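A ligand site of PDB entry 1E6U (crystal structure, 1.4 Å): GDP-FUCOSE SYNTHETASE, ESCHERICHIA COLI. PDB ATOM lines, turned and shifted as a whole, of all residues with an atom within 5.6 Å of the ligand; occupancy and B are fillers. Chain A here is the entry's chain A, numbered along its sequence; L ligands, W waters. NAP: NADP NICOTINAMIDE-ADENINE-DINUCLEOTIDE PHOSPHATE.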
ATOM      1  N   GLY A  10      16.932  14.557 -31.954  1.00  0.00           N
ATOM      2  CA  GLY A  10      16.449  14.223 -30.624  1.00  0.00           C
ATOM      3  C   GLY A  10      15.163  14.920 -30.209  1.00  0.00           C
ATOM      4  O   GLY A  10      14.917  15.296 -29.081  1.00  0.00           O
ATOM      5  N   HIS A  11      14.262  15.129 -31.213  1.00  0.00           N
ATOM      6  CA  HIS A  11      13.062  15.908 -30.951  1.00  0.00           C
ATOM      7  C   HIS A  11      12.023  15.337 -29.991  1.00  0.00           C
ATOM      8  O   HIS A  11      11.156  16.132 -29.609  1.00  0.00           O
ATOM      9  CB  HIS A  11      12.345  16.165 -32.315  1.00  0.00           C
ATOM     10  CG  HIS A  11      11.640  14.985 -32.872  1.00  0.00           C
ATOM     11  ND1 HIS A  11      12.282  13.987 -33.555  1.00  0.00           N
ATOM     12  CD2 HIS A  11      10.309  14.662 -32.877  1.00  0.00           C
ATOM     13  CE1 HIS A  11      11.405  13.071 -33.944  1.00  0.00           C
ATOM     14  NE2 HIS A  11      10.198  13.450 -33.510  1.00  0.00           N
ATOM     15  N   ARG A  12      12.124  14.068 -29.626  1.00  0.00           N
ATOM     16  CA  ARG A  12      11.239  13.527 -28.616  1.00  0.00           C
ATOM     17  C   ARG A  12      11.862  13.623 -27.224  1.00  0.00           C
ATOM     18  O   ARG A  12      11.208  13.259 -26.241  1.00  0.00           O
ATOM     19  CB  ARG A  12      10.871  12.050 -28.896  1.00  0.00           C
ATOM     20  CG  ARG A  12      10.040  11.878 -30.174  1.00  0.00           C
ATOM     21  CD  ARG A  12       9.573  10.430 -30.361  1.00  0.00           C
ATOM     22  NE  ARG A  12       8.505  10.391 -31.370  1.00  0.00           N
ATOM     23  CZ  ARG A  12       8.084   9.215 -31.829  1.00  0.00           C
ATOM     24  NH1 ARG A  12       8.664   8.126 -31.346  1.00  0.00           N
ATOM     25  NH2 ARG A  12       7.140   9.151 -32.747  1.00  0.00           N
ATOM     26  N   GLY A  13      13.098  14.114 -27.137  1.00  0.00           N
ATOM     27  CA  GLY A  13      13.709  14.258 -25.827  1.00  0.00           C
ATOM     28  C   GLY A  13      13.102  15.415 -25.063  1.00  0.00           C
ATOM     29  O   GLY A  13      12.253  16.221 -25.543  1.00  0.00           O
ATOM     30  N   MET A  14      13.528  15.567 -23.816  1.00  0.00           N
ATOM     31  CA  MET A  14      13.003  16.687 -23.025  1.00  0.00           C
ATOM     32  C   MET A  14      13.263  18.043 -23.625  1.00  0.00           C
ATOM     33  O   MET A  14      12.377  18.889 -23.825  1.00  0.00           O
ATOM     34  CB  MET A  14      13.545  16.548 -21.597  1.00  0.00           C
ATOM     35  CG  MET A  14      12.962  17.571 -20.656  1.00  0.00           C
ATOM     36  SD  MET A  14      13.483  17.157 -18.967  1.00  0.00           S
ATOM     37  CE  MET A  14      13.000  18.644 -18.236  1.00  0.00           C
ATOM     38  N   VAL A  15      14.532  18.308 -23.971  1.00  0.00           N
ATOM     39  CA  VAL A  15      14.910  19.604 -24.544  1.00  0.00           C
ATOM     40  C   VAL A  15      14.444  19.700 -26.003  1.00  0.00           C
ATOM     41  O   VAL A  15      13.870  20.719 -26.411  1.00  0.00           O
ATOM     42  CB  VAL A  15      16.427  19.792 -24.437  1.00  0.00           C
ATOM     43  CG1 VAL A  15      16.816  21.075 -25.151  1.00  0.00           C
ATOM     44  CG2 VAL A  15      16.868  19.926 -22.973  1.00  0.00           C
ATOM     45  N   GLY A  16      14.658  18.632 -26.762  1.00  0.00           N
ATOM     46  CA  GLY A  16      14.274  18.660 -28.186  1.00  0.00           C
ATOM     47  C   GLY A  16      12.801  18.932 -28.354  1.00  0.00           C
ATOM     48  O   GLY A  16      12.390  19.710 -29.248  1.00  0.00           O
ATOM     49  N   THR A  35      12.542  10.076 -35.882  1.00  0.00           N
ATOM     50  CA  THR A  35      12.676   9.360 -34.624  1.00  0.00           C
ATOM     51  C   THR A  35      13.949   8.498 -34.715  1.00  0.00           C
ATOM     52  O   THR A  35      14.541   8.282 -35.767  1.00  0.00           O
ATOM     53  CB  THR A  35      11.463   8.432 -34.447  1.00  0.00           C
ATOM     54  OG1 THR A  35      11.524   7.432 -35.460  1.00  0.00           O
ATOM     55  CG2 THR A  35      10.154   9.186 -34.473  1.00  0.00           C
ATOM     56  N   ARG A  36      14.328   7.946 -33.560  1.00  0.00           N
ATOM     57  CA  ARG A  36      15.498   7.068 -33.524  1.00  0.00           C
ATOM     58  C   ARG A  36      15.305   5.853 -34.419  1.00  0.00           C
ATOM     59  O   ARG A  36      16.218   5.451 -35.147  1.00  0.00           O
ATOM     60  CB  ARG A  36      15.726   6.598 -32.078  1.00  0.00           C
ATOM     61  CG  ARG A  36      16.946   5.686 -31.962  1.00  0.00           C
ATOM     62  CD  ARG A  36      17.519   5.671 -30.546  1.00  0.00           C
ATOM     63  NE  ARG A  36      18.773   4.894 -30.557  1.00  0.00           N
ATOM     64  CZ  ARG A  36      19.545   4.873 -29.469  1.00  0.00           C
ATOM     65  NH1 ARG A  36      19.104   5.590 -28.428  1.00  0.00           N
ATOM     66  NH2 ARG A  36      20.690   4.178 -29.447  1.00  0.00           N
ATOM     67  N   LEU A  39      16.094   7.145 -37.934  1.00  0.00           N
ATOM     68  CA  LEU A  39      17.459   7.597 -38.170  1.00  0.00           C
ATOM     69  C   LEU A  39      18.294   7.379 -36.904  1.00  0.00           C
ATOM     70  O   LEU A  39      18.083   8.099 -35.922  1.00  0.00           O
ATOM     71  CB  LEU A  39      17.474   9.069 -38.551  1.00  0.00           C
ATOM     72  CG  LEU A  39      18.864   9.710 -38.738  1.00  0.00           C
ATOM     73  CD1 LEU A  39      19.674   8.952 -39.780  1.00  0.00           C
ATOM     74  CD2 LEU A  39      18.732  11.175 -39.083  1.00  0.00           C
ATOM     75  N   ASN A  40      19.191   6.437 -36.957  1.00  0.00           N
ATOM     76  CA  ASN A  40      20.096   6.146 -35.844  1.00  0.00           C
ATOM     77  C   ASN A  40      21.320   7.050 -35.982  1.00  0.00           C
ATOM     78  O   ASN A  40      22.093   6.936 -36.916  1.00  0.00           O
ATOM     79  CB  ASN A  40      20.533   4.680 -35.868  1.00  0.00           C
ATOM     80  CG  ASN A  40      21.472   4.264 -34.746  1.00  0.00           C
ATOM     81  OD1 ASN A  40      21.872   3.088 -34.617  1.00  0.00           O
ATOM     82  ND2 ASN A  40      21.833   5.210 -33.948  1.00  0.00           N
ATOM     83  N   LEU A  41      21.372   8.071 -35.117  1.00  0.00           N
ATOM     84  CA  LEU A  41      22.407   9.089 -35.208  1.00  0.00           C
ATOM     85  C   LEU A  41      23.814   8.599 -34.930  1.00  0.00           C
ATOM     86  O   LEU A  41      24.790   9.320 -35.202  1.00  0.00           O
ATOM     87  CB  LEU A  41      22.058  10.283 -34.342  1.00  0.00           C
ATOM     88  CG  LEU A  41      20.722  10.945 -34.699  1.00  0.00           C
ATOM     89  CD1 LEU A  41      20.319  11.868 -33.585  1.00  0.00           C
ATOM     90  CD2 LEU A  41      20.799  11.719 -36.020  1.00  0.00           C
ATOM     91  N   LEU A  42      23.947   7.355 -34.454  1.00  0.00           N
ATOM     92  CA  LEU A  42      25.258   6.729 -34.323  1.00  0.00           C
ATOM     93  C   LEU A  42      25.817   6.224 -35.666  1.00  0.00           C
ATOM     94  O   LEU A  42      27.012   5.912 -35.746  1.00  0.00           O
ATOM     95  CB  LEU A  42      25.158   5.532 -33.346  1.00  0.00           C
ATOM     96  CG  LEU A  42      24.775   5.920 -31.910  1.00  0.00           C
ATOM     97  CD1 LEU A  42      24.399   4.688 -31.081  1.00  0.00           C
ATOM     98  CD2 LEU A  42      25.972   6.593 -31.261  1.00  0.00           C
ATOM     99  N   ALA A  62      19.935  18.249 -30.245  1.00  0.00           N
ATOM    100  CA  ALA A  62      19.349  17.933 -28.931  1.00  0.00           C
ATOM    101  C   ALA A  62      19.280  16.449 -28.700  1.00  0.00           C
ATOM    102  O   ALA A  62      18.579  15.974 -27.786  1.00  0.00           O
ATOM    103  CB  ALA A  62      17.987  18.612 -28.798  1.00  0.00           C
ATOM    104  N   ALA A  63      19.941  15.628 -29.521  1.00  0.00           N
ATOM    105  CA  ALA A  63      20.065  14.198 -29.342  1.00  0.00           C
ATOM    106  C   ALA A  63      21.306  13.897 -28.514  1.00  0.00           C
ATOM    107  O   ALA A  63      22.387  14.450 -28.780  1.00  0.00           O
ATOM    108  CB  ALA A  63      20.210  13.448 -30.655  1.00  0.00           C
ATOM    109  N   ALA A  64      21.190  12.998 -27.546  1.00  0.00           N
ATOM    110  CA  ALA A  64      22.297  12.648 -26.658  1.00  0.00           C
ATOM    111  C   ALA A  64      21.919  11.428 -25.836  1.00  0.00           C
ATOM    112  O   ALA A  64      20.712  11.133 -25.709  1.00  0.00           O
ATOM    113  CB  ALA A  64      22.587  13.789 -25.689  1.00  0.00           C
ATOM    114  N   LYS A  65      22.906  10.742 -25.310  1.00  0.00           N
ATOM    115  CA  LYS A  65      22.714   9.741 -24.272  1.00  0.00           C
ATOM    116  C   LYS A  65      22.880  10.480 -22.941  1.00  0.00           C
ATOM    117  O   LYS A  65      23.978  10.976 -22.645  1.00  0.00           O
ATOM    118  CB  LYS A  65      23.714   8.555 -24.383  1.00  0.00           C
ATOM    119  CG  LYS A  65      23.337   7.523 -23.300  1.00  0.00           C
ATOM    120  CD  LYS A  65      23.925   6.192 -23.176  1.00  0.00           C
ATOM    121  CE  LYS A  65      23.354   5.478 -21.979  1.00  0.00           C
ATOM    122  NZ  LYS A  65      21.980   4.931 -22.186  1.00  0.00           N
ATOM    123  N   VAL A  66      21.784  10.558 -22.197  1.00  0.00           N
ATOM    124  CA  VAL A  66      21.725  11.333 -20.943  1.00  0.00           C
ATOM    125  C   VAL A  66      21.194  10.451 -19.830  1.00  0.00           C
ATOM    126  O   VAL A  66      20.336   9.592 -20.110  1.00  0.00           O
ATOM    127  CB  VAL A  66      20.756  12.519 -21.178  1.00  0.00           C
ATOM    128  CG1 VAL A  66      20.667  13.471 -20.011  1.00  0.00           C
ATOM    129  CG2 VAL A  66      21.233  13.308 -22.384  1.00  0.00           C
ATOM    130  N   GLN A  82      28.765   7.133 -27.232  1.00  0.00           N
ATOM    131  CA  GLN A  82      27.563   7.476 -27.990  1.00  0.00           C
ATOM    132  C   GLN A  82      27.530   8.983 -28.215  1.00  0.00           C
ATOM    133  O   GLN A  82      27.147   9.419 -29.325  1.00  0.00           O
ATOM    134  CB  GLN A  82      26.270   6.954 -27.342  1.00  0.00           C
ATOM    135  CG  GLN A  82      26.181   5.454 -27.315  1.00  0.00           C
ATOM    136  CD  GLN A  82      24.921   4.941 -26.661  1.00  0.00           C
ATOM    137  OE1 GLN A  82      23.909   5.633 -26.691  1.00  0.00           O
ATOM    138  NE2 GLN A  82      25.058   3.732 -26.106  1.00  0.00           N
ATOM    139  N   ASN A  83      27.843   9.790 -27.228  1.00  0.00           N
ATOM    140  CA  ASN A  83      27.788  11.236 -27.411  1.00  0.00           C
ATOM    141  C   ASN A  83      28.882  11.685 -28.388  1.00  0.00           C
ATOM    142  O   ASN A  83      28.575  12.603 -29.155  1.00  0.00           O
ATOM    143  CB  ASN A  83      27.785  11.924 -26.069  1.00  0.00           C
ATOM    144  CG  ASN A  83      26.443  11.693 -25.355  1.00  0.00           C
ATOM    145  OD1 ASN A  83      25.407  12.129 -25.876  1.00  0.00           O
ATOM    146  ND2 ASN A  83      26.443  11.113 -24.184  1.00  0.00           N
ATOM    147  N   ILE A  86      27.462  10.665 -31.959  1.00  0.00           N
ATOM    148  CA  ILE A  86      26.294  11.436 -32.408  1.00  0.00           C
ATOM    149  C   ILE A  86      26.787  12.831 -32.816  1.00  0.00           C
ATOM    150  O   ILE A  86      26.405  13.355 -33.871  1.00  0.00           O
ATOM    151  CB  ILE A  86      25.269  11.579 -31.269  1.00  0.00           C
ATOM    152  CG1 ILE A  86      24.583  10.215 -31.069  1.00  0.00           C
ATOM    153  CG2 ILE A  86      24.226  12.644 -31.620  1.00  0.00           C
ATOM    154  CD1 ILE A  86      23.795  10.077 -29.775  1.00  0.00           C
ATOM    155  N   LEU A 105      24.001  21.579 -27.776  1.00  0.00           N
ATOM    156  CA  LEU A 105      23.756  21.673 -26.313  1.00  0.00           C
ATOM    157  C   LEU A 105      24.808  21.068 -25.414  1.00  0.00           C
ATOM    158  O   LEU A 105      25.069  19.853 -25.548  1.00  0.00           O
ATOM    159  CB  LEU A 105      22.488  20.955 -25.971  1.00  0.00           C
ATOM    160  CG  LEU A 105      21.320  21.346 -26.833  1.00  0.00           C
ATOM    161  CD1 LEU A 105      20.094  20.578 -26.369  1.00  0.00           C
ATOM    162  CD2 LEU A 105      21.039  22.835 -26.808  1.00  0.00           C
ATOM    163  N   GLY A 106      25.413  21.843 -24.569  1.00  0.00           N
ATOM    164  CA  GLY A 106      26.324  21.394 -23.529  1.00  0.00           C
ATOM    165  C   GLY A 106      25.473  21.007 -22.303  1.00  0.00           C
ATOM    166  O   GLY A 106      24.313  20.682 -22.361  1.00  0.00           O
ATOM    167  N   SER A 107      26.085  21.114 -21.192  1.00  0.00           N
ATOM    168  CA  SER A 107      25.515  20.755 -19.881  1.00  0.00           C
ATOM    169  C   SER A 107      26.430  21.467 -18.874  1.00  0.00           C
ATOM    170  O   SER A 107      27.631  21.566 -19.055  1.00  0.00           O
ATOM    171  CB  SER A 107      25.768  19.211 -19.788  1.00  0.00           C
ATOM    172  OG  SER A 107      25.150  18.857 -18.563  1.00  0.00           O
ATOM    173  N   SER A 108      25.857  21.949 -17.812  1.00  0.00           N
ATOM    174  CA  SER A 108      26.603  22.634 -16.758  1.00  0.00           C
ATOM    175  C   SER A 108      27.504  21.667 -16.002  1.00  0.00           C
ATOM    176  O   SER A 108      28.478  22.144 -15.395  1.00  0.00           O
ATOM    177  CB  SER A 108      25.644  23.373 -15.816  1.00  0.00           C
ATOM    178  OG  SER A 108      24.785  22.419 -15.222  1.00  0.00           O
ATOM    179  N   TYR A 136      30.825  11.595 -19.853  1.00  0.00           N
ATOM    180  CA  TYR A 136      29.831  12.416 -20.512  1.00  0.00           C
ATOM    181  C   TYR A 136      30.384  13.817 -20.769  1.00  0.00           C
ATOM    182  O   TYR A 136      30.188  14.390 -21.855  1.00  0.00           O
ATOM    183  CB  TYR A 136      28.576  12.431 -19.648  1.00  0.00           C
ATOM    184  CG  TYR A 136      27.496  13.355 -20.130  1.00  0.00           C
ATOM    185  CD1 TYR A 136      26.723  12.970 -21.202  1.00  0.00           C
ATOM    186  CD2 TYR A 136      27.152  14.530 -19.478  1.00  0.00           C
ATOM    187  CE1 TYR A 136      25.647  13.742 -21.629  1.00  0.00           C
ATOM    188  CE2 TYR A 136      26.083  15.302 -19.868  1.00  0.00           C
ATOM    189  CZ  TYR A 136      25.344  14.889 -20.963  1.00  0.00           C
ATOM    190  OH  TYR A 136      24.226  15.626 -21.332  1.00  0.00           O
ATOM    191  N   LYS A 140      30.866  15.992 -24.192  1.00  0.00           N
ATOM    192  CA  LYS A 140      30.227  17.286 -24.437  1.00  0.00           C
ATOM    193  C   LYS A 140      31.248  18.374 -24.717  1.00  0.00           C
ATOM    194  O   LYS A 140      31.010  19.191 -25.629  1.00  0.00           O
ATOM    195  CB  LYS A 140      29.355  17.697 -23.261  1.00  0.00           C
ATOM    196  CG  LYS A 140      28.081  16.880 -23.174  1.00  0.00           C
ATOM    197  CD  LYS A 140      27.138  17.117 -24.350  1.00  0.00           C
ATOM    198  CE  LYS A 140      25.713  16.735 -24.096  1.00  0.00           C
ATOM    199  NZ  LYS A 140      24.871  17.094 -25.301  1.00  0.00           N
ATOM    200  N   PRO A 163      23.269  24.721 -20.718  1.00  0.00           N
ATOM    201  CA  PRO A 163      22.171  24.901 -19.756  1.00  0.00           C
ATOM    202  C   PRO A 163      22.584  24.573 -18.329  1.00  0.00           C
ATOM    203  O   PRO A 163      23.423  23.715 -18.070  1.00  0.00           O
ATOM    204  CB  PRO A 163      21.148  23.861 -20.171  1.00  0.00           C
ATOM    205  CG  PRO A 163      21.896  22.850 -20.988  1.00  0.00           C
ATOM    206  CD  PRO A 163      23.098  23.556 -21.555  1.00  0.00           C
ATOM    207  N   THR A 164      21.908  25.187 -17.392  1.00  0.00           N
ATOM    208  CA  THR A 164      21.978  24.810 -15.964  1.00  0.00           C
ATOM    209  C   THR A 164      21.060  23.612 -15.760  1.00  0.00           C
ATOM    210  O   THR A 164      20.577  22.980 -16.726  1.00  0.00           O
ATOM    211  CB  THR A 164      21.600  26.002 -15.096  1.00  0.00           C
ATOM    212  OG1 THR A 164      22.016  25.748 -13.777  1.00  0.00           O
ATOM    213  CG2 THR A 164      20.155  26.410 -15.191  1.00  0.00           C
ATOM    214  N   ASN A 165      20.774  23.273 -14.493  1.00  0.00           N
ATOM    215  CA  ASN A 165      19.829  22.159 -14.244  1.00  0.00           C
ATOM    216  C   ASN A 165      18.452  22.523 -14.815  1.00  0.00           C
ATOM    217  O   ASN A 165      17.939  23.603 -14.543  1.00  0.00           O
ATOM    218  CB  ASN A 165      19.692  21.980 -12.702  1.00  0.00           C
ATOM    219  CG  ASN A 165      21.032  21.626 -12.094  1.00  0.00           C
ATOM    220  OD1 ASN A 165      21.618  20.584 -12.441  1.00  0.00           O
ATOM    221  ND2 ASN A 165      21.454  22.468 -11.171  1.00  0.00           N
ATOM    222  N   LEU A 166      17.896  21.569 -15.541  1.00  0.00           N
ATOM    223  CA  LEU A 166      16.607  21.789 -16.196  1.00  0.00           C
ATOM    224  C   LEU A 166      15.521  20.925 -15.544  1.00  0.00           C
ATOM    225  O   LEU A 166      15.802  19.875 -14.921  1.00  0.00           O
ATOM    226  CB  LEU A 166      16.682  21.412 -17.678  1.00  0.00           C
ATOM    227  CG  LEU A 166      17.728  22.157 -18.476  1.00  0.00           C
ATOM    228  CD1 LEU A 166      17.686  21.770 -19.960  1.00  0.00           C
ATOM    229  CD2 LEU A 166      17.555  23.682 -18.342  1.00  0.00           C
ATOM    230  N   HIS A 170       8.041  16.231 -19.763  1.00  0.00           N
ATOM    231  CA  HIS A 170       8.798  15.186 -20.414  1.00  0.00           C
ATOM    232  C   HIS A 170      10.042  14.733 -19.690  1.00  0.00           C
ATOM    233  O   HIS A 170      10.894  14.026 -20.234  1.00  0.00           O
ATOM    234  CB  HIS A 170       9.086  15.453 -21.908  1.00  0.00           C
ATOM    235  CG  HIS A 170       7.836  15.505 -22.724  1.00  0.00           C
ATOM    236  ND1 HIS A 170       7.087  14.407 -23.068  1.00  0.00           N
ATOM    237  CD2 HIS A 170       7.132  16.615 -23.082  1.00  0.00           C
ATOM    238  CE1 HIS A 170       6.021  14.828 -23.737  1.00  0.00           C
ATOM    239  NE2 HIS A 170       6.002  16.155 -23.719  1.00  0.00           N
HETATM  240  PA  NAP L   1      16.615  13.138 -23.417  1.00  0.00           P
HETATM  241  O1A NAP L   1      17.097  11.973 -22.833  1.00  0.00           O
HETATM  242  O2A NAP L   1      15.297  13.710 -22.911  1.00  0.00           O
HETATM  243  O5B NAP L   1      16.623  13.238 -24.934  1.00  0.00           O
HETATM  244  C5B NAP L   1      17.677  12.960 -25.844  1.00  0.00           C
HETATM  245  C4B NAP L   1      16.994  12.406 -27.141  1.00  0.00           C
HETATM  246  O4B NAP L   1      18.035  11.932 -28.049  1.00  0.00           O
HETATM  247  C3B NAP L   1      16.059  11.203 -26.939  1.00  0.00           C
HETATM  248  O3B NAP L   1      14.838  11.404 -27.612  1.00  0.00           O
HETATM  249  C2B NAP L   1      16.573  10.147 -27.969  1.00  0.00           C
HETATM  250  O2B NAP L   1      16.002   8.926 -28.098  1.00  0.00           O
HETATM  251  C1B NAP L   1      17.601  10.802 -28.746  1.00  0.00           C
HETATM  252  N9A NAP L   1      18.734   9.989 -29.110  1.00  0.00           N
HETATM  253  C8A NAP L   1      19.755   9.463 -28.331  1.00  0.00           C
HETATM  254  N7A NAP L   1      20.531   8.641 -29.034  1.00  0.00           N
HETATM  255  C5A NAP L   1      20.038   8.677 -30.331  1.00  0.00           C
HETATM  256  C6A NAP L   1      20.411   7.966 -31.504  1.00  0.00           C
HETATM  257  N6A NAP L   1      21.450   7.108 -31.552  1.00  0.00           N
HETATM  258  N1A NAP L   1      19.700   8.230 -32.624  1.00  0.00           N
HETATM  259  C2A NAP L   1      18.639   9.050 -32.564  1.00  0.00           C
HETATM  260  N3A NAP L   1      18.151   9.662 -31.478  1.00  0.00           N
HETATM  261  C4A NAP L   1      18.900   9.453 -30.375  1.00  0.00           C
HETATM  262  O3  NAP L   1      17.729  14.109 -23.023  1.00  0.00           O
HETATM  263  PN  NAP L   1      17.537  15.695 -22.608  1.00  0.00           P
HETATM  264  O1N NAP L   1      17.252  15.834 -21.144  1.00  0.00           O
HETATM  265  O2N NAP L   1      16.570  16.365 -23.582  1.00  0.00           O
HETATM  266  O5D NAP L   1      18.958  16.263 -22.809  1.00  0.00           O
HETATM  267  C5D NAP L   1      19.514  16.601 -24.071  1.00  0.00           C
HETATM  268  C4D NAP L   1      20.727  17.484 -23.925  1.00  0.00           C
HETATM  269  O4D NAP L   1      20.224  18.688 -23.297  1.00  0.00           O
HETATM  270  C3D NAP L   1      21.740  17.030 -22.877  1.00  0.00           C
HETATM  271  O3D NAP L   1      22.675  16.197 -23.542  1.00  0.00           O
HETATM  272  C2D NAP L   1      22.451  18.319 -22.414  1.00  0.00           C
HETATM  273  O2D NAP L   1      23.318  18.798 -23.490  1.00  0.00           O
HETATM  274  C1D NAP L   1      21.228  19.180 -22.465  1.00  0.00           C
HETATM  275  N1N NAP L   1      20.788  19.248 -21.102  1.00  0.00           N
HETATM  276  C2N NAP L   1      21.569  19.865 -20.134  1.00  0.00           C
HETATM  277  C3N NAP L   1      21.135  19.956 -18.763  1.00  0.00           C
HETATM  278  C4N NAP L   1      20.069  19.099 -18.431  1.00  0.00           C
HETATM  279  C5N NAP L   1      19.389  18.361 -19.438  1.00  0.00           C
HETATM  280  C6N NAP L   1      19.817  18.422 -20.770  1.00  0.00           C
HETATM  281  P2B NAP L   1      15.747   7.676 -27.207  1.00  0.00           P
HETATM  282  O1X NAP L   1      14.821   6.833 -27.956  1.00  0.00           O
HETATM  283  O2X NAP L   1      17.113   7.085 -26.891  1.00  0.00           O
HETATM  284  O3X NAP L   1      15.273   8.049 -25.863  1.00  0.00           O
HETATM  285  O   HOH W   1      14.017  11.851 -30.239  1.00  0.00           O
HETATM  286  O   HOH W   2      16.843  10.360 -35.177  1.00  0.00           O
HETATM  287  O   HOH W   3      19.194  19.014 -15.785  1.00  0.00           O
HETATM  288  O   HOH W   4      23.022  16.949 -19.438  1.00  0.00           O
HETATM  289  O   HOH W   5      16.241  16.369 -26.269  1.00  0.00           O
HETATM  290  O   HOH W   6      22.510   6.705 -28.832  1.00  0.00           O
HETATM  291  O   HOH W   7      19.312   7.594 -25.438  1.00  0.00           O
HETATM  292  O   HOH W   8      19.235   9.891 -23.620  1.00  0.00           O
HETATM  293  O   HOH W   9      16.998  11.484 -19.870  1.00  0.00           O
HETATM  294  O   HOH W  10      13.240  12.704 -20.306  1.00  0.00           O
HETATM  295  O   HOH W  11      13.168   9.882 -26.353  1.00  0.00           O
HETATM  296  O   HOH W  12      13.561  11.685 -22.566  1.00  0.00           O
HETATM  297  O   HOH W  13      15.912  11.265 -32.068  1.00  0.00           O
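O2D of the ligand is in hydrogen-bond range of O of Gly 106, 2.4 Å away. O2A of the ligand lies within hydrogen-bond range of N of Met 14. The side-chain hydroxyl (OH) of Tyr 136 lies within hydrogen-bond range of an oxygen (O3D) of the ligand, at 2.8 Å. The backbone NH of Val 15 is in hydrogen-bond range of an oxygen (O2N) of the ligand, 2.8 Å away. O of Leu 105 sits at hydrogen-bond distance from O2D of the ligand, at 2.9 Å. NH1 of Arg 36 lies within salt-bridge range of O2X of the ligand (2.9 Å). The side-chain amino group (NZ) of Lys 140 is in hydrogen-bond range of an oxygen (O2D) of the ligand (2.9 Å). N of Leu 41 is in hydrogen-bond range of N1A of the ligand (3.0 Å). The side-chain amide nitrogen of Asn 40 sits close to a nitrogen (N6A) of the ligand (3.1 Å). The backbone NH (N) of Gly 13 is in hydrogen-bond range of an oxygen (O3B) of the ligand (3.3 Å). N of Ala 64 sits at hydrogen-bond distance from O4B of the ligand (3.4 Å).
NZ of Lys 140 is in hydrogen-bond range of O of Leu 105 (2.8 Å). N of Leu 42 sits close to ND2 of Asn 40, 3.1 Å away. O of Pro 163 is in hydrogen-bond range of N of Ser 108, 3.0 Å away.
Gly 10 touches the ligand (CA to O4B, 3.8 Å). Arg 12 touches the ligand. Leu 39 touches the ligand. Leu 42 touches the ligand (CG to N6A, 3.5 Å). O of Ala 62 touches C5B of the ligand (3.7 Å). Ala 63 touches the ligand. Val 66 touches the ligand (CG2 to O3D, 3.4 Å). CD1 of Ile 86 touches N7A of the ligand, at 3.6 Å. Pro 163 touches the ligand (CG to C2N, 3.1 Å). Thr 164 touches the ligand (O to C3N, 3.7 Å). Leu 166 touches the ligand. Of the 32 residues printed, 22 come within 4 Å of the ligand.
Water W5 lies within hydrogen-bond range of O2N of the ligand (2.7 Å), N of Gly 16 (2.8 Å), O of Ala 62 (2.8 Å), O of Gly 10 (3.3 Å) and N of Val 15 (3.5 Å). Water W6 lies within hydrogen-bond range of the side-chain amide oxygen of Gln 82 (2.8 Å), a nitrogen (N7A) of the ligand (2.8 Å) and the guanidinium group of Arg 36 (3.2 Å). Water W1 lies within hydrogen-bond range of an oxygen (O3B) of the ligand (2.8 Å), the backbone NH of Arg 12 (3.0 Å) and the backbone NH of His 11 (3.4 Å). Water W13 lies within hydrogen-bond range of N3A of the ligand (2.8 Å) and N of Gly 10 (3.4 Å). Water W8 lies within hydrogen-bond range of O of Ala 64, N of Val 66 and O1A of the ligand. Water W4 bridges OH of Tyr 136 (2.6 Å) and OG of Ser 107 (3.0 Å).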
